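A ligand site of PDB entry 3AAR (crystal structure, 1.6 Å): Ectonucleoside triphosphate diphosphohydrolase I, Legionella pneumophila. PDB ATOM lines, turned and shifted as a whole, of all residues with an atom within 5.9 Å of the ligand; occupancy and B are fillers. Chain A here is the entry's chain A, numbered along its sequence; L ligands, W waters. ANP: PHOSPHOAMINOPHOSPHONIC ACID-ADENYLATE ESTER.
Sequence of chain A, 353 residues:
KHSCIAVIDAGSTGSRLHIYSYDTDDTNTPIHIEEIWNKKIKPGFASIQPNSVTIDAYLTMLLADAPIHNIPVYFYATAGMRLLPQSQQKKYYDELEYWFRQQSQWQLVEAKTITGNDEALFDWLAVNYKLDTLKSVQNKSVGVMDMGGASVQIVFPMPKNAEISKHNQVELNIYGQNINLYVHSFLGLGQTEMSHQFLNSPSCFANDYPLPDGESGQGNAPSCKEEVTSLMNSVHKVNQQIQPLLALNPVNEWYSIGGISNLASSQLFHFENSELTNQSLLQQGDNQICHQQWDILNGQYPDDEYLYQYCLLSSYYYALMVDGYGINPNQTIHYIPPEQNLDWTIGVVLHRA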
ATOM      1  N   GLY A  11       6.579 -13.794  16.396  1.00  0.00           N
ATOM      2  CA  GLY A  11       7.316 -14.963  15.915  1.00  0.00           C
ATOM      3  C   GLY A  11       6.540 -15.823  14.942  1.00  0.00           C
ATOM      4  O   GLY A  11       5.444 -15.469  14.502  1.00  0.00           O
ATOM      5  N   SER A  12       7.093 -16.992  14.634  1.00  0.00           N
ATOM      6  CA  SER A  12       6.561 -17.824  13.548  1.00  0.00           C
ATOM      7  C   SER A  12       5.186 -18.406  13.804  1.00  0.00           C
ATOM      8  O   SER A  12       4.297 -18.318  12.940  1.00  0.00           O
ATOM      9  CB  SER A  12       7.542 -18.952  13.221  1.00  0.00           C
ATOM     10  OG  SER A  12       8.817 -18.411  12.916  1.00  0.00           O
ATOM     11  N   THR A  13       5.002 -19.000  14.988  1.00  0.00           N
ATOM     12  CA  THR A  13       3.756 -19.692  15.335  1.00  0.00           C
ATOM     13  C   THR A  13       2.734 -18.784  16.017  1.00  0.00           C
ATOM     14  O   THR A  13       1.574 -19.165  16.214  1.00  0.00           O
ATOM     15  CB  THR A  13       4.021 -20.913  16.254  1.00  0.00           C
ATOM     16  OG1 THR A  13       4.574 -20.466  17.500  1.00  0.00           O
ATOM     17  CG2 THR A  13       4.962 -21.875  15.577  1.00  0.00           C
ATOM     18  N   GLY A  14       3.167 -17.576  16.363  1.00  0.00           N
ATOM     19  CA  GLY A  14       2.323 -16.683  17.123  1.00  0.00           C
ATOM     20  C   GLY A  14       3.059 -15.455  17.620  1.00  0.00           C
ATOM     21  O   GLY A  14       4.262 -15.335  17.432  1.00  0.00           O
ATOM     22  N   ARG A  16       3.777 -12.981  21.018  1.00  0.00           N
ATOM     23  CA  ARG A  16       3.728 -12.943  22.481  1.00  0.00           C
ATOM     24  C   ARG A  16       4.043 -11.534  22.983  1.00  0.00           C
ATOM     25  O   ARG A  16       5.110 -11.000  22.684  1.00  0.00           O
ATOM     26  CB  ARG A  16       4.695 -13.945  23.096  1.00  0.00           C
ATOM     27  CG  ARG A  16       4.496 -14.059  24.614  1.00  0.00           C
ATOM     28  CD  ARG A  16       5.419 -15.113  25.255  1.00  0.00           C
ATOM     29  NE  ARG A  16       5.024 -16.485  24.925  1.00  0.00           N
ATOM     30  CZ  ARG A  16       5.646 -17.264  24.050  1.00  0.00           C
ATOM     31  NH1 ARG A  16       6.709 -16.826  23.382  1.00  0.00           N
ATOM     32  NH2 ARG A  16       5.202 -18.505  23.842  1.00  0.00           N
ATOM     33  N   LYS A  40      -0.068 -14.673  24.646  1.00  0.00           N
ATOM     34  CA  LYS A  40       0.324 -15.298  23.386  1.00  0.00           C
ATOM     35  C   LYS A  40      -0.938 -15.472  22.563  1.00  0.00           C
ATOM     36  O   LYS A  40      -1.965 -15.935  23.078  1.00  0.00           O
ATOM     37  CB  LYS A  40       0.971 -16.670  23.661  1.00  0.00           C
ATOM     38  CG  LYS A  40       1.129 -17.592  22.451  1.00  0.00           C
ATOM     39  CD  LYS A  40       2.217 -17.151  21.514  1.00  0.00           C
ATOM     40  CE  LYS A  40       2.357 -18.095  20.309  1.00  0.00           C
ATOM     41  NZ  LYS A  40       3.023 -19.405  20.600  1.00  0.00           N
ATOM     42  N   ASP A 146      21.310 -19.892  19.893  1.00  0.00           N
ATOM     43  CA  ASP A 146      19.874 -20.138  19.868  1.00  0.00           C
ATOM     44  C   ASP A 146      19.545 -21.111  18.752  1.00  0.00           C
ATOM     45  O   ASP A 146      19.765 -20.822  17.564  1.00  0.00           O
ATOM     46  CB  ASP A 146      19.084 -18.821  19.662  1.00  0.00           C
ATOM     47  CG  ASP A 146      17.588 -19.055  19.597  1.00  0.00           C
ATOM     48  OD1 ASP A 146      17.104 -20.113  20.086  1.00  0.00           O
ATOM     49  OD2 ASP A 146      16.863 -18.185  19.051  1.00  0.00           O
ATOM     50  N   MET A 147      19.034 -22.277  19.149  1.00  0.00           N
ATOM     51  CA  MET A 147      18.534 -23.255  18.184  1.00  0.00           C
ATOM     52  C   MET A 147      17.043 -22.957  17.934  1.00  0.00           C
ATOM     53  O   MET A 147      16.138 -23.620  18.481  1.00  0.00           O
ATOM     54  CB  MET A 147      18.752 -24.702  18.697  1.00  0.00           C
ATOM     55  CG  MET A 147      20.185 -25.236  18.493  1.00  0.00           C
ATOM     56  SD  MET A 147      21.505 -24.162  19.112  1.00  0.00           S
ATOM     57  CE  MET A 147      22.923 -25.275  19.018  1.00  0.00           C
ATOM     58  N   GLY A 148      16.797 -21.941  17.112  1.00  0.00           N
ATOM     59  CA  GLY A 148      15.464 -21.511  16.826  1.00  0.00           C
ATOM     60  C   GLY A 148      14.728 -22.390  15.829  1.00  0.00           C
ATOM     61  O   GLY A 148      15.306 -23.308  15.246  1.00  0.00           O
ATOM     62  N   GLY A 149      13.447 -22.110  15.671  1.00  0.00           N
ATOM     63  CA  GLY A 149      12.632 -22.888  14.766  1.00  0.00           C
ATOM     64  C   GLY A 149      12.864 -22.547  13.313  1.00  0.00           C
ATOM     65  O   GLY A 149      12.813 -23.413  12.436  1.00  0.00           O
ATOM     66  N   ALA A 150      13.137 -21.268  13.025  1.00  0.00           N
ATOM     67  CA  ALA A 150      13.310 -20.840  11.632  1.00  0.00           C
ATOM     68  C   ALA A 150      14.716 -20.311  11.331  1.00  0.00           C
ATOM     69  O   ALA A 150      15.233 -20.514  10.229  1.00  0.00           O
ATOM     70  CB  ALA A 150      12.238 -19.807  11.233  1.00  0.00           C
ATOM     71  N   GLN A 191      15.381 -25.340  13.149  1.00  0.00           N
ATOM     72  CA  GLN A 191      15.065 -26.778  13.016  1.00  0.00           C
ATOM     73  C   GLN A 191      13.755 -27.099  12.270  1.00  0.00           C
ATOM     74  O   GLN A 191      13.690 -28.113  11.550  1.00  0.00           O
ATOM     75  CB  GLN A 191      15.107 -27.450  14.373  1.00  0.00           C
ATOM     76  CG  GLN A 191      14.239 -26.810  15.393  1.00  0.00           C
ATOM     77  CD  GLN A 191      14.395 -27.504  16.727  1.00  0.00           C
ATOM     78  OE1 GLN A 191      13.547 -28.336  17.089  1.00  0.00           O
ATOM     79  NE2 GLN A 191      15.467 -27.199  17.460  1.00  0.00           N
ATOM     80  N   THR A 192      12.738 -26.250  12.406  1.00  0.00           N
ATOM     81  CA  THR A 192      11.480 -26.482  11.670  1.00  0.00           C
ATOM     82  C   THR A 192      11.711 -26.285  10.184  1.00  0.00           C
ATOM     83  O   THR A 192      11.380 -27.152   9.377  1.00  0.00           O
ATOM     84  CB  THR A 192      10.345 -25.558  12.136  1.00  0.00           C
ATOM     85  OG1 THR A 192      10.124 -25.764  13.537  1.00  0.00           O
ATOM     86  CG2 THR A 192       9.050 -25.831  11.372  1.00  0.00           C
ATOM     87  N   GLY A 258      16.556 -22.638  23.026  1.00  0.00           N
ATOM     88  CA  GLY A 258      15.798 -23.149  21.872  1.00  0.00           C
ATOM     89  C   GLY A 258      15.586 -24.647  21.964  1.00  0.00           C
ATOM     90  O   GLY A 258      15.559 -25.221  23.059  1.00  0.00           O
ATOM     91  N   GLY A 259      15.443 -25.283  20.802  1.00  0.00           N
ATOM     92  CA  GLY A 259      14.928 -26.661  20.762  1.00  0.00           C
ATOM     93  C   GLY A 259      15.811 -27.669  21.465  1.00  0.00           C
ATOM     94  O   GLY A 259      15.320 -28.677  21.986  1.00  0.00           O
ATOM     95  N   ILE A 260      17.111 -27.398  21.439  1.00  0.00           N
ATOM     96  CA  ILE A 260      18.093 -28.318  22.029  1.00  0.00           C
ATOM     97  C   ILE A 260      17.822 -28.519  23.515  1.00  0.00           C
ATOM     98  O   ILE A 260      18.014 -29.610  24.048  1.00  0.00           O
ATOM     99  CB  ILE A 260      19.541 -27.865  21.739  1.00  0.00           C
ATOM    100  CG1 ILE A 260      20.537 -28.939  22.175  1.00  0.00           C
ATOM    101  CG2 ILE A 260      19.837 -26.470  22.360  1.00  0.00           C
ATOM    102  CD1 ILE A 260      21.875 -28.784  21.596  1.00  0.00           C
ATOM    103  N   ASN A 262      14.935 -28.545  24.918  1.00  0.00           N
ATOM    104  CA  ASN A 262      13.797 -29.427  24.998  1.00  0.00           C
ATOM    105  C   ASN A 262      14.207 -30.878  24.723  1.00  0.00           C
ATOM    106  O   ASN A 262      13.809 -31.794  25.464  1.00  0.00           O
ATOM    107  CB  ASN A 262      12.728 -28.985  24.008  1.00  0.00           C
ATOM    108  CG  ASN A 262      12.187 -27.615  24.321  1.00  0.00           C
ATOM    109  OD1 ASN A 262      11.382 -27.453  25.233  1.00  0.00           O
ATOM    110  ND2 ASN A 262      12.673 -26.610  23.598  1.00  0.00           N
ATOM    111  N   LEU A 263      15.020 -31.091  23.693  1.00  0.00           N
ATOM    112  CA  LEU A 263      15.505 -32.437  23.373  1.00  0.00           C
ATOM    113  C   LEU A 263      16.328 -32.975  24.541  1.00  0.00           C
ATOM    114  O   LEU A 263      16.165 -34.134  24.934  1.00  0.00           O
ATOM    115  CB  LEU A 263      16.332 -32.444  22.078  1.00  0.00           C
ATOM    116  CG  LEU A 263      16.919 -33.816  21.715  1.00  0.00           C
ATOM    117  CD1 LEU A 263      16.956 -33.968  20.191  1.00  0.00           C
ATOM    118  CD2 LEU A 263      18.329 -33.922  22.298  1.00  0.00           C
ATOM    119  N   SER A 266      14.348 -34.206  27.505  1.00  0.00           N
ATOM    120  CA  SER A 266      13.397 -35.280  27.224  1.00  0.00           C
ATOM    121  C   SER A 266      13.719 -36.537  28.021  1.00  0.00           C
ATOM    122  O   SER A 266      14.834 -36.697  28.541  1.00  0.00           O
ATOM    123  CB  SER A 266      13.369 -35.596  25.722  1.00  0.00           C
ATOM    124  OG  SER A 266      14.554 -36.268  25.329  1.00  0.00           O
ATOM    125  N   ASP A 304       5.693 -38.227  23.482  1.00  0.00           N
ATOM    126  CA  ASP A 304       6.668 -37.228  23.047  1.00  0.00           C
ATOM    127  C   ASP A 304       6.464 -36.988  21.555  1.00  0.00           C
ATOM    128  O   ASP A 304       6.812 -37.847  20.739  1.00  0.00           O
ATOM    129  CB  ASP A 304       8.111 -37.655  23.370  1.00  0.00           C
ATOM    130  CG  ASP A 304       9.123 -36.531  23.177  1.00  0.00           C
ATOM    131  OD1 ASP A 304       8.835 -35.616  22.371  1.00  0.00           O
ATOM    132  OD2 ASP A 304      10.200 -36.559  23.825  1.00  0.00           O
ATOM    133  N   TYR A 306       7.884 -35.029  19.536  1.00  0.00           N
ATOM    134  CA  TYR A 306       9.095 -34.790  18.755  1.00  0.00           C
ATOM    135  C   TYR A 306       9.932 -36.045  18.622  1.00  0.00           C
ATOM    136  O   TYR A 306      10.968 -36.021  17.975  1.00  0.00           O
ATOM    137  CB  TYR A 306       9.951 -33.676  19.374  1.00  0.00           C
ATOM    138  CG  TYR A 306       9.385 -32.303  19.143  1.00  0.00           C
ATOM    139  CD1 TYR A 306       9.890 -31.477  18.134  1.00  0.00           C
ATOM    140  CD2 TYR A 306       8.326 -31.822  19.921  1.00  0.00           C
ATOM    141  CE1 TYR A 306       9.348 -30.186  17.914  1.00  0.00           C
ATOM    142  CE2 TYR A 306       7.783 -30.564  19.709  1.00  0.00           C
ATOM    143  CZ  TYR A 306       8.300 -29.754  18.711  1.00  0.00           C
ATOM    144  OH  TYR A 306       7.760 -28.507  18.508  1.00  0.00           O
ATOM    145  N   TYR A 310      13.993 -37.248  16.590  1.00  0.00           N
ATOM    146  CA  TYR A 310      15.201 -37.175  17.420  1.00  0.00           C
ATOM    147  C   TYR A 310      16.472 -37.679  16.773  1.00  0.00           C
ATOM    148  O   TYR A 310      17.563 -37.290  17.196  1.00  0.00           O
ATOM    149  CB  TYR A 310      15.002 -37.824  18.806  1.00  0.00           C
ATOM    150  CG  TYR A 310      14.166 -37.016  19.788  1.00  0.00           C
ATOM    151  CD1 TYR A 310      14.023 -35.628  19.659  1.00  0.00           C
ATOM    152  CD2 TYR A 310      13.582 -37.640  20.888  1.00  0.00           C
ATOM    153  CE1 TYR A 310      13.270 -34.903  20.610  1.00  0.00           C
ATOM    154  CE2 TYR A 310      12.840 -36.937  21.822  1.00  0.00           C
ATOM    155  CZ  TYR A 310      12.700 -35.581  21.679  1.00  0.00           C
ATOM    156  OH  TYR A 310      11.953 -34.916  22.629  1.00  0.00           O
ATOM    157  N   LEU A 313      17.286 -34.528  14.687  1.00  0.00           N
ATOM    158  CA  LEU A 313      17.634 -33.354  15.490  1.00  0.00           C
ATOM    159  C   LEU A 313      18.977 -33.518  16.194  1.00  0.00           C
ATOM    160  O   LEU A 313      19.776 -32.589  16.223  1.00  0.00           O
ATOM    161  CB  LEU A 313      16.513 -33.009  16.465  1.00  0.00           C
ATOM    162  CG  LEU A 313      15.222 -32.419  15.845  1.00  0.00           C
ATOM    163  CD1 LEU A 313      14.206 -32.143  16.932  1.00  0.00           C
ATOM    164  CD2 LEU A 313      15.534 -31.149  15.031  1.00  0.00           C
ATOM    165  N   TYR A 317      21.953 -30.898  15.405  1.00  0.00           N
ATOM    166  CA  TYR A 317      22.637 -30.084  16.417  1.00  0.00           C
ATOM    167  C   TYR A 317      24.133 -30.313  16.369  1.00  0.00           C
ATOM    168  O   TYR A 317      24.907 -29.370  16.453  1.00  0.00           O
ATOM    169  CB  TYR A 317      22.131 -30.360  17.838  1.00  0.00           C
ATOM    170  CG  TYR A 317      20.677 -30.029  18.080  1.00  0.00           C
ATOM    171  CD1 TYR A 317      20.107 -28.831  17.628  1.00  0.00           C
ATOM    172  CD2 TYR A 317      19.864 -30.910  18.809  1.00  0.00           C
ATOM    173  CE1 TYR A 317      18.757 -28.544  17.881  1.00  0.00           C
ATOM    174  CE2 TYR A 317      18.547 -30.633  19.050  1.00  0.00           C
ATOM    175  CZ  TYR A 317      17.977 -29.455  18.588  1.00  0.00           C
ATOM    176  OH  TYR A 317      16.658 -29.189  18.861  1.00  0.00           O
HETATM  177  PG  ANP L   1       8.178 -20.396  17.487  1.00  0.00           P
HETATM  178  O1G ANP L   1       8.596 -20.988  16.219  1.00  0.00           O
HETATM  179  O2G ANP L   1       6.948 -19.344  17.271  1.00  0.00           O
HETATM  180  O3G ANP L   1       9.349 -19.547  18.126  1.00  0.00           O
HETATM  181  PB  ANP L   1       8.052 -21.727  20.080  1.00  0.00           P
HETATM  182  O1B ANP L   1       7.219 -22.620  20.804  1.00  0.00           O
HETATM  183  O2B ANP L   1       8.383 -20.446  20.728  1.00  0.00           O
HETATM  184  N3B ANP L   1       7.797 -21.682  18.479  1.00  0.00           N
HETATM  185  PA  ANP L   1      10.756 -22.136  20.928  1.00  0.00           P
HETATM  186  O1A ANP L   1      10.503 -22.033  22.323  1.00  0.00           O
HETATM  187  O2A ANP L   1      11.524 -21.006  20.295  1.00  0.00           O
HETATM  188  O3A ANP L   1       9.541 -22.486  20.022  1.00  0.00           O
HETATM  189  O5' ANP L   1      11.818 -23.347  20.642  1.00  0.00           O
HETATM  190  C5' ANP L   1      12.659 -23.439  19.475  1.00  0.00           C
HETATM  191  C4' ANP L   1      12.399 -24.741  18.695  1.00  0.00           C
HETATM  192  O4' ANP L   1      12.444 -25.965  19.554  1.00  0.00           O
HETATM  193  C3' ANP L   1      10.976 -24.757  18.096  1.00  0.00           C
HETATM  194  O3' ANP L   1      11.110 -25.231  16.791  1.00  0.00           O
HETATM  195  C2' ANP L   1      10.204 -25.796  18.919  1.00  0.00           C
HETATM  196  O2' ANP L   1       9.341 -26.502  18.084  1.00  0.00           O
HETATM  197  C1' ANP L   1      11.300 -26.766  19.311  1.00  0.00           C
HETATM  198  N9  ANP L   1      10.990 -27.918  20.258  1.00  0.00           N
HETATM  199  C8  ANP L   1       9.949 -28.072  21.087  1.00  0.00           C
HETATM  200  N7  ANP L   1      10.026 -29.222  21.727  1.00  0.00           N
HETATM  201  C5  ANP L   1      11.112 -29.853  21.287  1.00  0.00           C
HETATM  202  C6  ANP L   1      11.720 -31.092  21.568  1.00  0.00           C
HETATM  203  N6  ANP L   1      11.204 -31.947  22.446  1.00  0.00           N
HETATM  204  N1  ANP L   1      12.841 -31.375  20.920  1.00  0.00           N
HETATM  205  C2  ANP L   1      13.392 -30.557  20.043  1.00  0.00           C
HETATM  206  N3  ANP L   1      12.834 -29.406  19.747  1.00  0.00           N
HETATM  207  C4  ANP L   1      11.718 -29.029  20.345  1.00  0.00           C
HETATM  208  O   HOH W   1       6.146 -17.331  18.689  1.00  0.00           O
HETATM  209  O   HOH W   2       5.148 -20.995  22.703  1.00  0.00           O
HETATM  210  O   HOH W   3       4.557 -22.902  20.056  1.00  0.00           O
HETATM  211  O   HOH W   4      12.059 -18.281  18.941  1.00  0.00           O
HETATM  212  O   HOH W   5       8.773 -33.141  23.525  1.00  0.00           O
HETATM  213  O   HOH W   6      11.878 -20.293  17.010  1.00  0.00           O
HETATM  214  O   HOH W   7      10.496 -20.115  14.424  1.00  0.00           O
HETATM  215  O   HOH W   8       8.325 -23.819  14.576  1.00  0.00           O
HETATM  216  O   HOH W   9       8.012 -24.833  23.179  1.00  0.00           O
HETATM  217  O   HOH W  10       9.366 -17.446  16.473  1.00  0.00           O
HETATM  218  O   HOH W  11       8.794 -16.714  19.789  1.00  0.00           O
HETATM  219  O   HOH W  12       6.189 -18.747  21.050  1.00  0.00           O
HETATM  220  O   HOH W  13      14.479 -20.074  20.600  1.00  0.00           O
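The side-chain hydroxyl of Thr 13 lies within hydrogen-bond range of an oxygen (O2G) of the ligand (2.6 Å).
O2' of the ligand sits at hydrogen-bond distance from OH of Tyr 306, 2.6 Å away.
N of Thr 13 is in hydrogen-bond range of O2G of the ligand (3.0 Å).
The side-chain hydroxyl (OH) of Tyr 310 lies within hydrogen-bond range of a nitrogen (N6) of the ligand, 3.1 Å away.
The side-chain hydroxyl (OG1) of Thr 192 lies within hydrogen-bond range of an oxygen (O3') of the ligand (3.4 Å).
The backbone NH (N) of Gly 259 sits close to an oxygen (O4') of the ligand, 3.3 Å away.
A nitrogen (N3) of the ligand lies close to the side-chain amide oxygen (OE1) of Gln 191, at 3.0 Å.
The side-chain amide nitrogen of Gln 191 is in hydrogen-bond range of the side-chain hydroxyl of Tyr 317, at 2.7 Å.
The side-chain hydroxyl (OH) of Tyr 317 lies close to the backbone carbonyl oxygen (O) of Gly 259.
The side-chain hydroxyl of Tyr 310 sits at hydrogen-bond distance from the side-chain carboxylate of Asp 304.
The backbone carbonyl oxygen of Gly 149 lies within hydrogen-bond range of the backbone NH of Gln 191 (3.3 Å).
The side-chain carboxylate of Asp 304 sits at hydrogen-bond distance from the backbone NH of Tyr 306 (3.0 Å).
N of Gln 191 is in hydrogen-bond range of O of Gly 148 (2.9 Å).
The side-chain amide nitrogen (ND2) of Asn 262 sits at hydrogen-bond distance from the backbone carbonyl oxygen (O) of Gly 258, 3.2 Å away.
OH of Tyr 317 lies within hydrogen-bond range of N of Ile 260 (3.2 Å).
Residues that only touch the ligand: Asn 262, Gly 149, Ser 12, Leu 263, Leu 313, Met 147, Tyr 317 and Gly 258.
14 residues have an atom within 4 Å of the ligand: Ser 12, Thr 13, Met 147, Gly 149, Gln 191, Thr 192, Gly 258, Gly 259, Asn 262, Leu 263, Tyr 306, Tyr 310, Leu 313 and Tyr 317.
The nearest printed residue that does not touch the ligand is Gly 11 (4.2 Å).
Water W10 lies within hydrogen-bond range of O3G of the ligand (2.7 Å) and N of Ser 12 (3.0 Å).
Water W12 lies within hydrogen-bond range of O2B of the ligand, NH2 of Arg 16 and NZ of Lys 40.
Water W5 lies within hydrogen-bond range of the side-chain carboxylate of Asp 304 (2.7 Å) and a nitrogen (N6) of the ligand (2.9 Å).
Water W13 bridges OD1 of Asp 146 (2.7 Å) and O2A of the ligand (3.1 Å).
Water W2 lies within hydrogen-bond range of NH2 of Arg 16 (2.7 Å), O1B of the ligand (3.2 Å) and NZ of Lys 40 (3.4 Å).
Water W8 lies within hydrogen-bond range of OG1 of Thr 192 and O1G of the ligand.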
